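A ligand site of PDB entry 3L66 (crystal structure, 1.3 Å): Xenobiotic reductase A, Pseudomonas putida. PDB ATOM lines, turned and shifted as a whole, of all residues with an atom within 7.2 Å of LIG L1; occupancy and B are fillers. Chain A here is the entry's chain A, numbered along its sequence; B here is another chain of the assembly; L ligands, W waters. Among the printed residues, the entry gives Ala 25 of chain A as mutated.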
ATOM      1  N   PRO A  23      27.868   6.275  19.909  1.00  0.00           N
ATOM      2  CA  PRO A  23      28.167   5.458  21.071  1.00  0.00           C
ATOM      3  C   PRO A  23      27.095   4.398  21.317  1.00  0.00           C
ATOM      4  O   PRO A  23      25.888   4.692  21.326  1.00  0.00           O
ATOM      5  CB  PRO A  23      28.201   6.483  22.215  1.00  0.00           C
ATOM      6  CG  PRO A  23      27.323   7.628  21.721  1.00  0.00           C
ATOM      7  CD  PRO A  23      27.652   7.700  20.249  1.00  0.00           C
ATOM      8  N   MET A  24      27.543   3.161  21.514  1.00  0.00           N
ATOM      9  CA  MET A  24      26.636   2.061  21.822  1.00  0.00           C
ATOM     10  C   MET A  24      27.230   1.199  22.948  1.00  0.00           C
ATOM     11  O   MET A  24      28.123   0.357  22.704  1.00  0.00           O
ATOM     12  CB  MET A  24      26.341   1.215  20.580  1.00  0.00           C
ATOM     13  CG  MET A  24      25.374   1.920  19.618  1.00  0.00           C
ATOM     14  SD  MET A  24      25.012   0.866  18.162  1.00  0.00           S
ATOM     15  CE  MET A  24      26.577   0.933  17.335  1.00  0.00           C
ATOM     16  N   ALA A  25      26.697   1.404  24.138  1.00  0.00           N
ATOM     17  CA  ALA A  25      27.015   0.616  25.327  1.00  0.00           C
ATOM     18  C   ALA A  25      26.981  -0.882  25.026  1.00  0.00           C
ATOM     19  O   ALA A  25      26.035  -1.381  24.416  1.00  0.00           O
ATOM     20  CB  ALA A  25      26.050   0.948  26.424  1.00  0.00           C
ATOM     21  N   TYR A  27      28.019  -3.227  27.692  1.00  0.00           N
ATOM     22  CA  TYR A  27      27.719  -3.890  28.959  1.00  0.00           C
ATOM     23  C   TYR A  27      28.635  -5.098  29.192  1.00  0.00           C
ATOM     24  O   TYR A  27      28.227  -6.070  29.825  1.00  0.00           O
ATOM     25  CB  TYR A  27      26.241  -4.266  29.080  1.00  0.00           C
ATOM     26  CG  TYR A  27      25.293  -3.130  28.741  1.00  0.00           C
ATOM     27  CD1 TYR A  27      24.906  -2.219  29.720  1.00  0.00           C
ATOM     28  CD2 TYR A  27      24.859  -2.917  27.437  1.00  0.00           C
ATOM     29  CE1 TYR A  27      24.055  -1.159  29.415  1.00  0.00           C
ATOM     30  CE2 TYR A  27      24.008  -1.857  27.132  1.00  0.00           C
ATOM     31  CZ  TYR A  27      23.603  -1.003  28.116  1.00  0.00           C
ATOM     32  OH  TYR A  27      22.760   0.038  27.768  1.00  0.00           O
ATOM     33  N   ALA A  57      29.234   5.153  25.910  1.00  0.00           N
ATOM     34  CA  ALA A  57      29.205   5.893  27.188  1.00  0.00           C
ATOM     35  C   ALA A  57      30.228   5.319  28.166  1.00  0.00           C
ATOM     36  O   ALA A  57      30.057   4.199  28.637  1.00  0.00           O
ATOM     37  CB  ALA A  57      27.804   5.878  27.791  1.00  0.00           C
ATOM     38  N   ILE A  66      26.141   3.335  34.026  1.00  0.00           N
ATOM     39  CA  ILE A  66      24.732   2.942  34.009  1.00  0.00           C
ATOM     40  C   ILE A  66      24.605   1.624  34.759  1.00  0.00           C
ATOM     41  O   ILE A  66      23.682   1.449  35.573  1.00  0.00           O
ATOM     42  CB  ILE A  66      24.213   2.786  32.575  1.00  0.00           C
ATOM     43  CG1 ILE A  66      24.496   4.032  31.722  1.00  0.00           C
ATOM     44  CG2 ILE A  66      22.691   2.518  32.611  1.00  0.00           C
ATOM     45  CD1 ILE A  66      24.355   3.765  30.239  1.00  0.00           C
ATOM     46  N   GLN A  99      32.575   8.908  24.013  1.00  0.00           N
ATOM     47  CA  GLN A  99      31.555   9.619  24.773  1.00  0.00           C
ATOM     48  C   GLN A  99      31.843   9.429  26.262  1.00  0.00           C
ATOM     49  O   GLN A  99      31.870   8.299  26.741  1.00  0.00           O
ATOM     50  CB  GLN A  99      30.156   9.084  24.415  1.00  0.00           C
ATOM     51  CG  GLN A  99      29.058   9.861  25.112  1.00  0.00           C
ATOM     52  CD  GLN A  99      27.713   9.189  24.957  1.00  0.00           C
ATOM     53  OE1 GLN A  99      27.516   8.055  25.429  1.00  0.00           O
ATOM     54  NE2 GLN A  99      26.749   9.906  24.363  1.00  0.00           N
ATOM     55  N   PRO A 112      20.690  -4.619  30.086  1.00  0.00           N
ATOM     56  CA  PRO A 112      19.355  -4.640  29.471  1.00  0.00           C
ATOM     57  C   PRO A 112      18.781  -6.046  29.312  1.00  0.00           C
ATOM     58  O   PRO A 112      17.573  -6.210  29.437  1.00  0.00           O
ATOM     59  CB  PRO A 112      19.587  -3.969  28.127  1.00  0.00           C
ATOM     60  CG  PRO A 112      20.716  -2.957  28.441  1.00  0.00           C
ATOM     61  CD  PRO A 112      21.630  -3.771  29.306  1.00  0.00           C
ATOM     62  N   ASP A 116      17.140  -4.890  33.034  1.00  0.00           N
ATOM     63  CA  ASP A 116      17.129  -3.485  32.594  1.00  0.00           C
ATOM     64  C   ASP A 116      16.641  -2.492  33.672  1.00  0.00           C
ATOM     65  O   ASP A 116      16.440  -1.310  33.369  1.00  0.00           O
ATOM     66  CB  ASP A 116      16.252  -3.311  31.351  1.00  0.00           C
ATOM     67  CG  ASP A 116      16.577  -2.063  30.558  1.00  0.00           C
ATOM     68  OD1 ASP A 116      17.775  -1.817  30.351  1.00  0.00           O
ATOM     69  OD2 ASP A 116      15.603  -1.373  30.105  1.00  0.00           O
ATOM     70  N   HIS A 178      28.318  13.486  27.316  1.00  0.00           N
ATOM     71  CA  HIS A 178      26.966  12.895  27.334  1.00  0.00           C
ATOM     72  C   HIS A 178      26.013  13.684  28.204  1.00  0.00           C
ATOM     73  O   HIS A 178      25.856  13.409  29.400  1.00  0.00           O
ATOM     74  CB  HIS A 178      27.010  11.461  27.828  1.00  0.00           C
ATOM     75  CG  HIS A 178      25.813  10.669  27.465  1.00  0.00           C
ATOM     76  ND1 HIS A 178      24.694  11.243  26.918  1.00  0.00           N
ATOM     77  CD2 HIS A 178      25.590   9.339  27.493  1.00  0.00           C
ATOM     78  CE1 HIS A 178      23.824  10.289  26.632  1.00  0.00           C
ATOM     79  NE2 HIS A 178      24.358   9.119  26.949  1.00  0.00           N
ATOM     80  N   ALA A 180      22.794  13.893  27.356  1.00  0.00           N
ATOM     81  CA  ALA A 180      21.492  13.448  26.830  1.00  0.00           C
ATOM     82  C   ALA A 180      20.922  12.265  27.614  1.00  0.00           C
ATOM     83  O   ALA A 180      21.507  11.785  28.587  1.00  0.00           O
ATOM     84  CB  ALA A 180      21.629  13.117  25.330  1.00  0.00           C
ATOM     85  N   HIS A 181      19.704  11.869  27.241  1.00  0.00           N
ATOM     86  CA  HIS A 181      19.132  10.562  27.602  1.00  0.00           C
ATOM     87  C   HIS A 181      18.813  10.398  29.073  1.00  0.00           C
ATOM     88  O   HIS A 181      18.691   9.268  29.579  1.00  0.00           O
ATOM     89  CB  HIS A 181      20.018   9.427  27.065  1.00  0.00           C
ATOM     90  CG  HIS A 181      20.176   9.482  25.584  1.00  0.00           C
ATOM     91  ND1 HIS A 181      21.056   8.668  24.887  1.00  0.00           N
ATOM     92  CD2 HIS A 181      19.536  10.226  24.643  1.00  0.00           C
ATOM     93  CE1 HIS A 181      20.968   8.936  23.599  1.00  0.00           C
ATOM     94  NE2 HIS A 181      20.066   9.879  23.435  1.00  0.00           N
ATOM     95  N   GLY A 182      18.630  11.524  29.751  1.00  0.00           N
ATOM     96  CA  GLY A 182      18.122  11.534  31.112  1.00  0.00           C
ATOM     97  C   GLY A 182      19.154  11.261  32.187  1.00  0.00           C
ATOM     98  O   GLY A 182      18.826  11.108  33.362  1.00  0.00           O
ATOM     99  N   TYR A 183      20.404  11.206  31.757  1.00  0.00           N
ATOM    100  CA  TYR A 183      21.543  10.998  32.648  1.00  0.00           C
ATOM    101  C   TYR A 183      21.881  12.315  33.333  1.00  0.00           C
ATOM    102  O   TYR A 183      21.064  13.248  33.352  1.00  0.00           O
ATOM    103  CB  TYR A 183      22.712  10.370  31.865  1.00  0.00           C
ATOM    104  CG  TYR A 183      22.354   9.036  31.238  1.00  0.00           C
ATOM    105  CD1 TYR A 183      21.809   8.003  31.979  1.00  0.00           C
ATOM    106  CD2 TYR A 183      22.545   8.809  29.900  1.00  0.00           C
ATOM    107  CE1 TYR A 183      21.505   6.756  31.415  1.00  0.00           C
ATOM    108  CE2 TYR A 183      22.216   7.565  29.304  1.00  0.00           C
ATOM    109  CZ  TYR A 183      21.693   6.567  30.050  1.00  0.00           C
ATOM    110  OH  TYR A 183      21.372   5.364  29.463  1.00  0.00           O
ATOM    111  N   ARG A 231      26.368  15.428  23.223  1.00  0.00           N
ATOM    112  CA  ARG A 231      25.052  14.897  22.906  1.00  0.00           C
ATOM    113  C   ARG A 231      24.066  15.504  23.893  1.00  0.00           C
ATOM    114  O   ARG A 231      24.333  15.540  25.093  1.00  0.00           O
ATOM    115  CB  ARG A 231      25.059  13.353  22.941  1.00  0.00           C
ATOM    116  CG  ARG A 231      23.853  12.764  22.222  1.00  0.00           C
ATOM    117  CD  ARG A 231      23.935  11.253  22.049  1.00  0.00           C
ATOM    118  NE  ARG A 231      23.156  10.883  20.874  1.00  0.00           N
ATOM    119  CZ  ARG A 231      23.072   9.658  20.372  1.00  0.00           C
ATOM    120  NH1 ARG A 231      22.437   9.444  19.212  1.00  0.00           N
ATOM    121  NH2 ARG A 231      23.569   8.615  21.031  1.00  0.00           N
ATOM    122  N   PHE A 269      14.655  11.762  27.113  1.00  0.00           N
ATOM    123  CA  PHE A 269      14.387  10.569  27.932  1.00  0.00           C
ATOM    124  C   PHE A 269      14.528  10.884  29.434  1.00  0.00           C
ATOM    125  O   PHE A 269      14.962  10.040  30.213  1.00  0.00           O
ATOM    126  CB  PHE A 269      15.295   9.364  27.560  1.00  0.00           C
ATOM    127  CG  PHE A 269      15.158   8.924  26.146  1.00  0.00           C
ATOM    128  CD1 PHE A 269      14.118   8.098  25.775  1.00  0.00           C
ATOM    129  CD2 PHE A 269      16.068   9.319  25.194  1.00  0.00           C
ATOM    130  CE1 PHE A 269      13.979   7.690  24.479  1.00  0.00           C
ATOM    131  CE2 PHE A 269      15.943   8.913  23.896  1.00  0.00           C
ATOM    132  CZ  PHE A 269      14.909   8.097  23.533  1.00  0.00           C
ATOM    133  N   TRP A 302      18.492   7.430  14.578  1.00  0.00           N
ATOM    134  CA  TRP A 302      17.271   6.634  14.714  1.00  0.00           C
ATOM    135  C   TRP A 302      16.722   6.315  13.327  1.00  0.00           C
ATOM    136  O   TRP A 302      15.988   7.147  12.720  1.00  0.00           O
ATOM    137  CB  TRP A 302      16.166   7.232  15.576  1.00  0.00           C
ATOM    138  CG  TRP A 302      15.056   6.217  15.742  1.00  0.00           C
ATOM    139  CD1 TRP A 302      13.997   5.951  14.879  1.00  0.00           C
ATOM    140  CD2 TRP A 302      14.920   5.294  16.825  1.00  0.00           C
ATOM    141  NE1 TRP A 302      13.215   4.978  15.389  1.00  0.00           N
ATOM    142  CE2 TRP A 302      13.763   4.533  16.572  1.00  0.00           C
ATOM    143  CE3 TRP A 302      15.622   5.093  18.013  1.00  0.00           C
ATOM    144  CZ2 TRP A 302      13.333   3.530  17.443  1.00  0.00           C
ATOM    145  CZ3 TRP A 302      15.200   4.083  18.874  1.00  0.00           C
ATOM    146  CH2 TRP A 302      14.068   3.325  18.589  1.00  0.00           C
ATOM    147  N   TRP B 358      19.260  -6.240  20.943  1.00  0.00           N
ATOM    148  CA  TRP B 358      18.766  -5.023  20.302  1.00  0.00           C
ATOM    149  C   TRP B 358      18.194  -5.253  18.917  1.00  0.00           C
ATOM    150  O   TRP B 358      17.633  -4.340  18.318  1.00  0.00           O
ATOM    151  CB  TRP B 358      19.943  -4.035  20.164  1.00  0.00           C
ATOM    152  CG  TRP B 358      20.601  -3.841  21.456  1.00  0.00           C
ATOM    153  CD1 TRP B 358      21.822  -4.321  21.826  1.00  0.00           C
ATOM    154  CD2 TRP B 358      20.055  -3.186  22.597  1.00  0.00           C
ATOM    155  NE1 TRP B 358      22.076  -4.012  23.135  1.00  0.00           N
ATOM    156  CE2 TRP B 358      21.007  -3.295  23.631  1.00  0.00           C
ATOM    157  CE3 TRP B 358      18.850  -2.517  22.860  1.00  0.00           C
ATOM    158  CZ2 TRP B 358      20.826  -2.718  24.872  1.00  0.00           C
ATOM    159  CZ3 TRP B 358      18.662  -1.969  24.124  1.00  0.00           C
ATOM    160  CH2 TRP B 358      19.653  -2.079  25.109  1.00  0.00           C
HETATM  161  C1  LIG L   1      22.362   5.607  26.180  1.00  0.00           C
HETATM  162  C2  LIG L   1      23.030   4.530  26.800  1.00  0.00           C
HETATM  163  C3  LIG L   1      22.625   3.216  26.557  1.00  0.00           C
HETATM  164  C4  LIG L   1      21.522   3.002  25.704  1.00  0.00           C
HETATM  165  C5  LIG L   1      21.045   1.718  25.376  1.00  0.00           C
HETATM  166  C6  LIG L   1      19.964   1.586  24.546  1.00  0.00           C
HETATM  167  C7  LIG L   1      19.344   2.709  23.981  1.00  0.00           C
HETATM  168  C8  LIG L   1      19.794   3.972  24.294  1.00  0.00           C
HETATM  169  C9  LIG L   1      20.883   4.104  25.130  1.00  0.00           C
HETATM  170  O1  LIG L   1      22.701   6.786  26.292  1.00  0.00           O
HETATM  171  O2  LIG L   1      21.286   5.386  25.373  1.00  0.00           O
HETATM  172  N1  LG2 L   2      23.415   6.448  23.098  1.00  0.00           N
HETATM  173  C1  LG2 L   2      24.299   7.190  23.780  1.00  0.00           C
HETATM  174  O1  LG2 L   2      24.351   8.409  23.787  1.00  0.00           O
HETATM  175  N2  LG2 L   2      25.310   6.466  24.476  1.00  0.00           N
HETATM  176  C2  LG2 L   2      25.393   5.137  24.535  1.00  0.00           C
HETATM  177  O2  LG2 L   2      26.403   4.574  25.092  1.00  0.00           O
HETATM  178  C3  LG2 L   2      24.326   4.422  23.958  1.00  0.00           C
HETATM  179  N3  LG2 L   2      24.392   3.031  24.005  1.00  0.00           N
HETATM  180  C4  LG2 L   2      23.499   2.370  23.160  1.00  0.00           C
HETATM  181  C5  LG2 L   2      23.605   0.974  23.171  1.00  0.00           C
HETATM  182  C6  LG2 L   2      22.907   0.186  22.218  1.00  0.00           C
HETATM  183  C7  LG2 L   2      23.163  -1.299  22.020  1.00  0.00           C
HETATM  184  C8  LG2 L   2      22.002   0.852  21.370  1.00  0.00           C
HETATM  185  C9  LG2 L   2      21.208   0.075  20.345  1.00  0.00           C
HETATM  186  C10 LG2 L   2      21.839   2.247  21.447  1.00  0.00           C
HETATM  187  C11 LG2 L   2      22.642   3.025  22.346  1.00  0.00           C
HETATM  188  N4  LG2 L   2      22.582   4.406  22.340  1.00  0.00           N
HETATM  189  C12 LG2 L   2      23.451   5.096  23.137  1.00  0.00           C
HETATM  190  C13 LG2 L   2      21.794   5.145  21.280  1.00  0.00           C
HETATM  191  C14 LG2 L   2      22.426   5.034  19.950  1.00  0.00           C
HETATM  192  O3  LG2 L   2      23.640   5.844  19.921  1.00  0.00           O
HETATM  193  C15 LG2 L   2      21.542   5.557  18.810  1.00  0.00           C
HETATM  194  O4  LG2 L   2      21.119   6.893  19.071  1.00  0.00           O
HETATM  195  C16 LG2 L   2      20.280   4.699  18.623  1.00  0.00           C
HETATM  196  O5  LG2 L   2      20.627   3.298  18.570  1.00  0.00           O
HETATM  197  C17 LG2 L   2      19.501   5.139  17.428  1.00  0.00           C
HETATM  198  O6  LG2 L   2      20.184   4.954  16.177  1.00  0.00           O
HETATM  199  P1  LG2 L   2      19.849   3.622  15.261  1.00  0.00           P
HETATM  200  O7  LG2 L   2      20.132   2.408  16.124  1.00  0.00           O
HETATM  201  O8  LG2 L   2      18.358   3.634  14.910  1.00  0.00           O
HETATM  202  O9  LG2 L   2      20.736   3.785  14.135  1.00  0.00           O
HETATM  203  O   HOH W   1      18.166   5.871  26.112  1.00  0.00           O
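A nitrogen (N2) of LG2 L2 lies close to an oxygen (O1) of LIG L1 (3.2 Å).
ND1 of His 181 lies within hydrogen-bond range of O1 of LIG L1. A ring nitrogen (NE2) of His 178 lies within hydrogen-bond range of an oxygen (O1) of LIG L1. O1 of LG2 L2 lies close to ND1 of His 181 (3.5 Å). A ring nitrogen (NE2) of His 178 is in hydrogen-bond range of an oxygen (O1) of LG2 L2 (3.2 Å). N of Ala 25 is in hydrogen-bond range of N3 of LG2 L2 (2.8 Å). The side-chain amide oxygen (OE1) of Gln 99 is in hydrogen-bond range of a nitrogen (N2) of LG2 L2 (2.9 Å). O2 of LG2 L2 lies within hydrogen-bond range of N of Ala 57, at 3.0 Å. The guanidinium group (NH2) of Arg 231 sits at hydrogen-bond distance from an oxygen (O1) of LG2 L2, 2.9 Å away. An oxygen (O3) of LG2 L2 sits at hydrogen-bond distance from the backbone carbonyl oxygen (O) of Pro 23. An oxygen (O6) of LG2 L2 sits at hydrogen-bond distance from the backbone NH (N) of Trp 302, 3.4 Å away.
ND1 of His 178 lies within hydrogen-bond range of N of Ala 180 (3.3 Å).
Merely in contact with LIG L1: Tyr 183 (3.1 Å), Tyr 27 (3.4 Å), Trp 358 of chain B (3.7 Å) and Ile 66 (3.8 Å). Hydrophobic or aromatic side chains that line LIG L1: Ile 66, His 178, His 181, Tyr 183 and Trp 358 of chain B. Six residues have an atom within 4 Å of LIG L1: Tyr 27, Ile 66, His 178, His 181, Tyr 183 and Trp 358 of chain B. Along chain A the residues within 4 Å of LIG L1 span positions 27 to 183. The nearest printed residue that does not touch LIG L1 is Ala 25 (4.1 Å).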
